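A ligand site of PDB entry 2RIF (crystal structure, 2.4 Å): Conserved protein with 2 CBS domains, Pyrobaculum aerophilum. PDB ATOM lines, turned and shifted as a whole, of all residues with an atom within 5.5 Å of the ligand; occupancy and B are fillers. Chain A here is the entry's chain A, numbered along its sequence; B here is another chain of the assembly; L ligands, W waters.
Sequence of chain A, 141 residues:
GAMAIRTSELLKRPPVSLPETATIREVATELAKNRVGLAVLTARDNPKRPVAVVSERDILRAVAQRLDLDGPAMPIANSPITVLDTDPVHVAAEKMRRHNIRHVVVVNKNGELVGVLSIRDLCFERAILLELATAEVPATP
N of Gly 37 sits at hydrogen-bond distance from O2 of the ligand (2.8 Å). O of Leu 38 sits at hydrogen-bond distance from N3 of the ligand (3.1 Å). The guanidinium group (NH2) of Arg 13 is in hydrogen-bond range of an oxygen (O5) of the ligand (3.1 Å). The guanidinium group (NH2) of Arg 57 of chain B lies within salt-bridge range of an oxygen (O1) of the ligand. The backbone NH (N) of Val 16 is in hydrogen-bond range of a nitrogen (N4) of the ligand, at 2.8 Å. An oxygen (O3) of the ligand is in hydrogen-bond range of the side-chain hydroxyl (OG) of Ser 118 (2.7 Å). The side-chain carboxylate (OD2) of Asp 121 sits at hydrogen-bond distance from an oxygen (O7) of the ligand (2.6 Å). NE2 of His 103 lies within hydrogen-bond range of O2 of the ligand. NH2 of Arg 120 is in salt-bridge range of O1 of the ligand (3.1 Å). O of Val 16 lies within hydrogen-bond range of N3 of the ligand.
Lys 12 touches the ligand. O of Pro 14 touches C9 of the ligand, 3.5 Å away. Pro 15 touches the ligand (CA to N4, 3.5 Å). Val 36 touches the ligand (CA to O2, 3.4 Å). CB of Val 116 touches C8 of the ligand, 3.4 Å away. Hydrophobic or aromatic side chains within 4 Å of the ligand: Val 16, Val 36, His 103 and Val 116.
Water W1 lies within hydrogen-bond range of an oxygen (O3) of the ligand, the side-chain hydroxyl of Ser 118 and the guanidinium group of Arg 102 of chain B.
N of Val 40 lies within hydrogen-bond range of O of Val 16, at 3.2 Å. NZ of Lys 12 lies close to O of Leu 10 (3.4 Å). The side-chain carboxylate of Asp 121 lies within salt-bridge range of the side-chain amino group of Lys 12 (3.4 Å). The backbone NH (N) of Arg 120 sits close to the side-chain hydroxyl (OG) of Ser 118, 3.0 Å away. OD2 of Asp 121 lies within hydrogen-bond range of N of Ser 118 (2.8 Å).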
ATOM      1  N   LEU A  10       7.206  -9.022  -9.059  1.00  0.00           N
ATOM      2  CA  LEU A  10       7.478  -8.583  -7.685  1.00  0.00           C
ATOM      3  C   LEU A  10       6.866  -7.204  -7.382  1.00  0.00           C
ATOM      4  O   LEU A  10       7.003  -6.710  -6.261  1.00  0.00           O
ATOM      5  CB  LEU A  10       8.984  -8.551  -7.410  1.00  0.00           C
ATOM      6  CG  LEU A  10       9.728  -9.885  -7.451  1.00  0.00           C
ATOM      7  CD1 LEU A  10      11.196  -9.683  -7.148  1.00  0.00           C
ATOM      8  CD2 LEU A  10       9.115 -10.883  -6.479  1.00  0.00           C
ATOM      9  N   LYS A  12       3.943  -4.872  -6.317  1.00  0.00           N
ATOM     10  CA  LYS A  12       2.710  -5.011  -5.540  1.00  0.00           C
ATOM     11  C   LYS A  12       2.017  -3.672  -5.234  1.00  0.00           C
ATOM     12  O   LYS A  12       1.029  -3.650  -4.485  1.00  0.00           O
ATOM     13  CB  LYS A  12       2.994  -5.749  -4.221  1.00  0.00           C
ATOM     14  CG  LYS A  12       4.095  -5.127  -3.358  1.00  0.00           C
ATOM     15  CD  LYS A  12       5.444  -5.797  -3.574  1.00  0.00           C
ATOM     16  CE  LYS A  12       5.537  -7.153  -2.869  1.00  0.00           C
ATOM     17  NZ  LYS A  12       6.887  -7.763  -3.010  1.00  0.00           N
ATOM     18  N   ARG A  13       2.494  -2.574  -5.824  1.00  0.00           N
ATOM     19  CA  ARG A  13       1.973  -1.243  -5.505  1.00  0.00           C
ATOM     20  C   ARG A  13       2.137  -0.270  -6.674  1.00  0.00           C
ATOM     21  O   ARG A  13       3.125  -0.345  -7.399  1.00  0.00           O
ATOM     22  CB  ARG A  13       2.703  -0.695  -4.280  1.00  0.00           C
ATOM     23  CG  ARG A  13       2.078   0.548  -3.658  1.00  0.00           C
ATOM     24  CD  ARG A  13       2.937   1.149  -2.537  1.00  0.00           C
ATOM     25  NE  ARG A  13       3.498   0.131  -1.633  1.00  0.00           N
ATOM     26  CZ  ARG A  13       3.944   0.371  -0.402  1.00  0.00           C
ATOM     27  NH1 ARG A  13       3.904   1.588   0.119  1.00  0.00           N
ATOM     28  NH2 ARG A  13       4.428  -0.635   0.318  1.00  0.00           N
ATOM     29  N   PRO A  14       1.159   0.643  -6.849  1.00  0.00           N
ATOM     30  CA  PRO A  14       1.326   1.695  -7.864  1.00  0.00           C
ATOM     31  C   PRO A  14       2.447   2.658  -7.488  1.00  0.00           C
ATOM     32  O   PRO A  14       2.635   2.941  -6.305  1.00  0.00           O
ATOM     33  CB  PRO A  14      -0.023   2.424  -7.851  1.00  0.00           C
ATOM     34  CG  PRO A  14      -0.965   1.539  -7.143  1.00  0.00           C
ATOM     35  CD  PRO A  14      -0.168   0.714  -6.205  1.00  0.00           C
ATOM     36  N   PRO A  15       3.194   3.179  -8.487  1.00  0.00           N
ATOM     37  CA  PRO A  15       4.361   4.021  -8.219  1.00  0.00           C
ATOM     38  C   PRO A  15       4.056   5.285  -7.412  1.00  0.00           C
ATOM     39  O   PRO A  15       3.124   6.024  -7.751  1.00  0.00           O
ATOM     40  CB  PRO A  15       4.852   4.395  -9.623  1.00  0.00           C
ATOM     41  CG  PRO A  15       3.680   4.203 -10.511  1.00  0.00           C
ATOM     42  CD  PRO A  15       2.909   3.061  -9.929  1.00  0.00           C
ATOM     43  N   VAL A  16       4.822   5.501  -6.352  1.00  0.00           N
ATOM     44  CA  VAL A  16       4.730   6.711  -5.545  1.00  0.00           C
ATOM     45  C   VAL A  16       5.573   7.775  -6.227  1.00  0.00           C
ATOM     46  O   VAL A  16       6.793   7.635  -6.325  1.00  0.00           O
ATOM     47  CB  VAL A  16       5.260   6.481  -4.119  1.00  0.00           C
ATOM     48  CG1 VAL A  16       5.296   7.787  -3.340  1.00  0.00           C
ATOM     49  CG2 VAL A  16       4.406   5.443  -3.397  1.00  0.00           C
ATOM     50  N   ARG A  35       4.805   5.585   3.348  1.00  0.00           N
ATOM     51  CA  ARG A  35       5.734   4.740   4.100  1.00  0.00           C
ATOM     52  C   ARG A  35       6.741   4.022   3.195  1.00  0.00           C
ATOM     53  O   ARG A  35       6.895   2.797   3.251  1.00  0.00           O
ATOM     54  CB  ARG A  35       4.978   3.739   5.000  1.00  0.00           C
ATOM     55  CG  ARG A  35       4.159   4.428   6.085  1.00  0.00           C
ATOM     56  CD  ARG A  35       3.507   3.424   7.016  1.00  0.00           C
ATOM     57  NE  ARG A  35       2.720   4.107   8.049  1.00  0.00           N
ATOM     58  CZ  ARG A  35       3.223   4.656   9.160  1.00  0.00           C
ATOM     59  NH1 ARG A  35       4.539   4.616   9.409  1.00  0.00           N
ATOM     60  NH2 ARG A  35       2.409   5.245  10.022  1.00  0.00           N
ATOM     61  N   VAL A  36       7.427   4.808   2.381  1.00  0.00           N
ATOM     62  CA  VAL A  36       8.435   4.305   1.452  1.00  0.00           C
ATOM     63  C   VAL A  36       9.717   5.120   1.574  1.00  0.00           C
ATOM     64  O   VAL A  36       9.727   6.208   2.137  1.00  0.00           O
ATOM     65  CB  VAL A  36       7.935   4.324  -0.009  1.00  0.00           C
ATOM     66  CG1 VAL A  36       6.708   3.430  -0.155  1.00  0.00           C
ATOM     67  CG2 VAL A  36       7.612   5.745  -0.445  1.00  0.00           C
ATOM     68  N   GLY A  37      10.808   4.579   1.032  1.00  0.00           N
ATOM     69  CA  GLY A  37      12.114   5.197   1.138  1.00  0.00           C
ATOM     70  C   GLY A  37      12.496   6.072  -0.042  1.00  0.00           C
ATOM     71  O   GLY A  37      13.412   6.883   0.066  1.00  0.00           O
ATOM     72  N   LEU A  38      11.792   5.909  -1.160  1.00  0.00           N
ATOM     73  CA  LEU A  38      12.113   6.623  -2.393  1.00  0.00           C
ATOM     74  C   LEU A  38      10.857   7.180  -3.037  1.00  0.00           C
ATOM     75  O   LEU A  38       9.771   6.623  -2.898  1.00  0.00           O
ATOM     76  CB  LEU A  38      12.799   5.658  -3.370  1.00  0.00           C
ATOM     77  CG  LEU A  38      13.472   6.254  -4.614  1.00  0.00           C
ATOM     78  CD1 LEU A  38      14.924   6.609  -4.335  1.00  0.00           C
ATOM     79  CD2 LEU A  38      13.379   5.274  -5.776  1.00  0.00           C
ATOM     80  N   ALA A  39      11.019   8.305  -3.741  1.00  0.00           N
ATOM     81  CA  ALA A  39       9.940   8.914  -4.526  1.00  0.00           C
ATOM     82  C   ALA A  39      10.468   9.242  -5.915  1.00  0.00           C
ATOM     83  O   ALA A  39      11.543   9.818  -6.049  1.00  0.00           O
ATOM     84  CB  ALA A  39       9.430  10.160  -3.843  1.00  0.00           C
ATOM     85  N   VAL A  40       9.703   8.874  -6.946  1.00  0.00           N
ATOM     86  CA  VAL A  40      10.087   9.142  -8.326  1.00  0.00           C
ATOM     87  C   VAL A  40       9.564  10.507  -8.739  1.00  0.00           C
ATOM     88  O   VAL A  40       8.379  10.794  -8.593  1.00  0.00           O
ATOM     89  CB  VAL A  40       9.506   8.077  -9.287  1.00  0.00           C
ATOM     90  CG1 VAL A  40       9.981   8.331 -10.702  1.00  0.00           C
ATOM     91  CG2 VAL A  40       9.900   6.675  -8.834  1.00  0.00           C
ATOM     92  N   ARG A 102      19.342   1.039  -2.767  1.00  0.00           N
ATOM     93  CA  ARG A 102      18.366   0.078  -2.254  1.00  0.00           C
ATOM     94  C   ARG A 102      17.044   0.164  -3.014  1.00  0.00           C
ATOM     95  O   ARG A 102      16.024  -0.360  -2.558  1.00  0.00           O
ATOM     96  CB  ARG A 102      18.141   0.332  -0.761  1.00  0.00           C
ATOM     97  CG  ARG A 102      19.406   0.117   0.083  1.00  0.00           C
ATOM     98  CD  ARG A 102      19.215   0.517   1.545  1.00  0.00           C
ATOM     99  NE  ARG A 102      18.919   1.944   1.694  1.00  0.00           N
ATOM    100  CZ  ARG A 102      18.842   2.588   2.853  1.00  0.00           C
ATOM    101  NH1 ARG A 102      19.027   1.960   4.009  1.00  0.00           N
ATOM    102  NH2 ARG A 102      18.559   3.881   2.853  1.00  0.00           N
ATOM    103  N   HIS A 103      17.065   0.813  -4.182  1.00  0.00           N
ATOM    104  CA  HIS A 103      15.890   0.915  -5.042  1.00  0.00           C
ATOM    105  C   HIS A 103      16.278   0.876  -6.521  1.00  0.00           C
ATOM    106  O   HIS A 103      17.390   1.254  -6.876  1.00  0.00           O
ATOM    107  CB  HIS A 103      15.116   2.217  -4.790  1.00  0.00           C
ATOM    108  CG  HIS A 103      14.532   2.324  -3.410  1.00  0.00           C
ATOM    109  ND1 HIS A 103      15.254   2.816  -2.341  1.00  0.00           N
ATOM    110  CD2 HIS A 103      13.300   2.020  -2.940  1.00  0.00           C
ATOM    111  CE1 HIS A 103      14.488   2.802  -1.262  1.00  0.00           C
ATOM    112  NE2 HIS A 103      13.300   2.330  -1.602  1.00  0.00           N
ATOM    113  N   GLY A 115       6.672   0.960 -12.094  1.00  0.00           N
ATOM    114  CA  GLY A 115       6.739   0.854 -10.646  1.00  0.00           C
ATOM    115  C   GLY A 115       8.150   1.018 -10.099  1.00  0.00           C
ATOM    116  O   GLY A 115       9.066   1.421 -10.830  1.00  0.00           O
ATOM    117  N   VAL A 116       8.308   0.724  -8.813  1.00  0.00           N
ATOM    118  CA  VAL A 116       9.601   0.822  -8.145  1.00  0.00           C
ATOM    119  C   VAL A 116       9.851  -0.432  -7.314  1.00  0.00           C
ATOM    120  O   VAL A 116       8.985  -0.848  -6.546  1.00  0.00           O
ATOM    121  CB  VAL A 116       9.681   2.054  -7.241  1.00  0.00           C
ATOM    122  CG1 VAL A 116      10.923   2.013  -6.352  1.00  0.00           C
ATOM    123  CG2 VAL A 116       9.647   3.328  -8.076  1.00  0.00           C
ATOM    124  N   LEU A 117      11.032  -1.017  -7.467  1.00  0.00           N
ATOM    125  CA  LEU A 117      11.425  -2.202  -6.732  1.00  0.00           C
ATOM    126  C   LEU A 117      12.422  -1.786  -5.652  1.00  0.00           C
ATOM    127  O   LEU A 117      13.182  -0.837  -5.847  1.00  0.00           O
ATOM    128  CB  LEU A 117      12.058  -3.216  -7.687  1.00  0.00           C
ATOM    129  CG  LEU A 117      11.843  -4.700  -7.388  1.00  0.00           C
ATOM    130  CD1 LEU A 117      10.361  -5.055  -7.385  1.00  0.00           C
ATOM    131  CD2 LEU A 117      12.588  -5.529  -8.428  1.00  0.00           C
ATOM    132  N   SER A 118      12.416  -2.503  -4.536  1.00  0.00           N
ATOM    133  CA  SER A 118      13.270  -2.193  -3.388  1.00  0.00           C
ATOM    134  C   SER A 118      14.076  -3.407  -2.959  1.00  0.00           C
ATOM    135  O   SER A 118      13.701  -4.548  -3.219  1.00  0.00           O
ATOM    136  CB  SER A 118      12.400  -1.716  -2.228  1.00  0.00           C
ATOM    137  OG  SER A 118      13.095  -1.741  -0.994  1.00  0.00           O
ATOM    138  N   ILE A 119      15.194  -3.154  -2.276  1.00  0.00           N
ATOM    139  CA  ILE A 119      16.013  -4.220  -1.695  1.00  0.00           C
ATOM    140  C   ILE A 119      15.195  -5.063  -0.705  1.00  0.00           C
ATOM    141  O   ILE A 119      15.511  -6.226  -0.455  1.00  0.00           O
ATOM    142  CB  ILE A 119      17.270  -3.643  -0.985  1.00  0.00           C
ATOM    143  CG1 ILE A 119      18.292  -4.735  -0.701  1.00  0.00           C
ATOM    144  CG2 ILE A 119      16.885  -2.914   0.295  1.00  0.00           C
ATOM    145  CD1 ILE A 119      19.636  -4.207  -0.240  1.00  0.00           C
ATOM    146  N   ARG A 120      14.153  -4.454  -0.145  1.00  0.00           N
ATOM    147  CA  ARG A 120      13.215  -5.136   0.747  1.00  0.00           C
ATOM    148  C   ARG A 120      12.457  -6.261   0.027  1.00  0.00           C
ATOM    149  O   ARG A 120      12.154  -7.292   0.626  1.00  0.00           O
ATOM    150  CB  ARG A 120      12.225  -4.108   1.310  1.00  0.00           C
ATOM    151  CG  ARG A 120      11.683  -4.440   2.682  1.00  0.00           C
ATOM    152  CD  ARG A 120      10.665  -3.393   3.125  1.00  0.00           C
ATOM    153  NE  ARG A 120      11.266  -2.076   3.317  1.00  0.00           N
ATOM    154  CZ  ARG A 120      11.821  -1.628   4.448  1.00  0.00           C
ATOM    155  NH1 ARG A 120      11.888  -2.392   5.535  1.00  0.00           N
ATOM    156  NH2 ARG A 120      12.337  -0.402   4.481  1.00  0.00           N
ATOM    157  N   ASP A 121      12.161  -6.052  -1.262  1.00  0.00           N
ATOM    158  CA  ASP A 121      11.435  -7.033  -2.077  1.00  0.00           C
ATOM    159  C   ASP A 121      12.267  -8.277  -2.403  1.00  0.00           C
ATOM    160  O   ASP A 121      11.730  -9.383  -2.460  1.00  0.00           O
ATOM    161  CB  ASP A 121      10.988  -6.405  -3.396  1.00  0.00           C
ATOM    162  CG  ASP A 121      10.057  -5.220  -3.204  1.00  0.00           C
ATOM    163  OD1 ASP A 121       9.157  -5.301  -2.344  1.00  0.00           O
ATOM    164  OD2 ASP A 121      10.229  -4.220  -3.930  1.00  0.00           O
ATOM    165  N   ARG B  57      14.945   7.180   8.334  1.00  0.00           N
ATOM    166  CA  ARG B  57      13.486   7.006   8.260  1.00  0.00           C
ATOM    167  C   ARG B  57      12.787   7.743   9.397  1.00  0.00           C
ATOM    168  O   ARG B  57      11.738   8.345   9.191  1.00  0.00           O
ATOM    169  CB  ARG B  57      13.143   5.500   8.317  1.00  0.00           C
ATOM    170  CG  ARG B  57      11.642   5.124   8.319  1.00  0.00           C
ATOM    171  CD  ARG B  57      10.919   5.391   6.990  1.00  0.00           C
ATOM    172  NE  ARG B  57      11.578   4.771   5.841  1.00  0.00           N
ATOM    173  CZ  ARG B  57      11.148   3.713   5.146  1.00  0.00           C
ATOM    174  NH1 ARG B  57      10.012   3.080   5.446  1.00  0.00           N
ATOM    175  NH2 ARG B  57      11.870   3.286   4.118  1.00  0.00           N
ATOM    176  N   ARG B 102      16.033  -2.668   8.303  1.00  0.00           N
ATOM    177  CA  ARG B 102      17.164  -2.891   7.415  1.00  0.00           C
ATOM    178  C   ARG B 102      18.492  -2.815   8.161  1.00  0.00           C
ATOM    179  O   ARG B 102      19.557  -2.728   7.547  1.00  0.00           O
ATOM    180  CB  ARG B 102      17.125  -1.894   6.263  1.00  0.00           C
ATOM    181  CG  ARG B 102      15.921  -2.063   5.362  1.00  0.00           C
ATOM    182  CD  ARG B 102      15.808  -0.940   4.343  1.00  0.00           C
ATOM    183  NE  ARG B 102      15.520   0.335   4.973  1.00  0.00           N
ATOM    184  CZ  ARG B 102      15.358   1.487   4.332  1.00  0.00           C
ATOM    185  NH1 ARG B 102      15.455   1.543   3.012  1.00  0.00           N
ATOM    186  NH2 ARG B 102      15.090   2.591   5.024  1.00  0.00           N
HETATM  187  P1  LIG L   1      10.811   0.876   1.051  1.00  0.00           P
HETATM  188  O1  LIG L   1      10.795   1.348   2.479  1.00  0.00           O
HETATM  189  O2  LIG L   1      10.519   1.980   0.056  1.00  0.00           O
HETATM  190  O3  LIG L   1      11.975  -0.004   0.680  1.00  0.00           O
HETATM  191  O4  LIG L   1       9.572  -0.136   1.024  1.00  0.00           O
HETATM  192  C1  LIG L   1       8.303   0.175   0.447  1.00  0.00           C
HETATM  193  C2  LIG L   1       7.829  -0.991  -0.414  1.00  0.00           C
HETATM  194  O5  LIG L   1       6.965  -0.485  -1.432  1.00  0.00           O
HETATM  195  C3  LIG L   1       8.957  -1.740  -1.090  1.00  0.00           C
HETATM  196  O6  LIG L   1       9.022  -3.086  -0.619  1.00  0.00           O
HETATM  197  C4  LIG L   1       8.653  -1.669  -2.581  1.00  0.00           C
HETATM  198  O7  LIG L   1       8.147  -2.908  -3.077  1.00  0.00           O
HETATM  199  C5  LIG L   1       7.579  -0.611  -2.706  1.00  0.00           C
HETATM  200  N1  LIG L   1       8.127   0.715  -3.110  1.00  0.00           N
HETATM  201  C6  LIG L   1       9.272   1.301  -2.711  1.00  0.00           C
HETATM  202  N2  LIG L   1       9.414   2.520  -3.287  1.00  0.00           N
HETATM  203  C7  LIG L   1       8.342   2.731  -4.065  1.00  0.00           C
HETATM  204  C8  LIG L   1       7.840   3.799  -4.955  1.00  0.00           C
HETATM  205  N3  LIG L   1       8.555   4.936  -5.144  1.00  0.00           N
HETATM  206  N4  LIG L   1       6.665   3.597  -5.593  1.00  0.00           N
HETATM  207  C9  LIG L   1       5.937   2.473  -5.420  1.00  0.00           C
HETATM  208  N5  LIG L   1       6.334   1.465  -4.628  1.00  0.00           N
HETATM  209  C10 LIG L   1       7.500   1.535  -3.943  1.00  0.00           C
HETATM  210  O   HOH W   1      14.599  -0.188   0.723  1.00  0.00           O
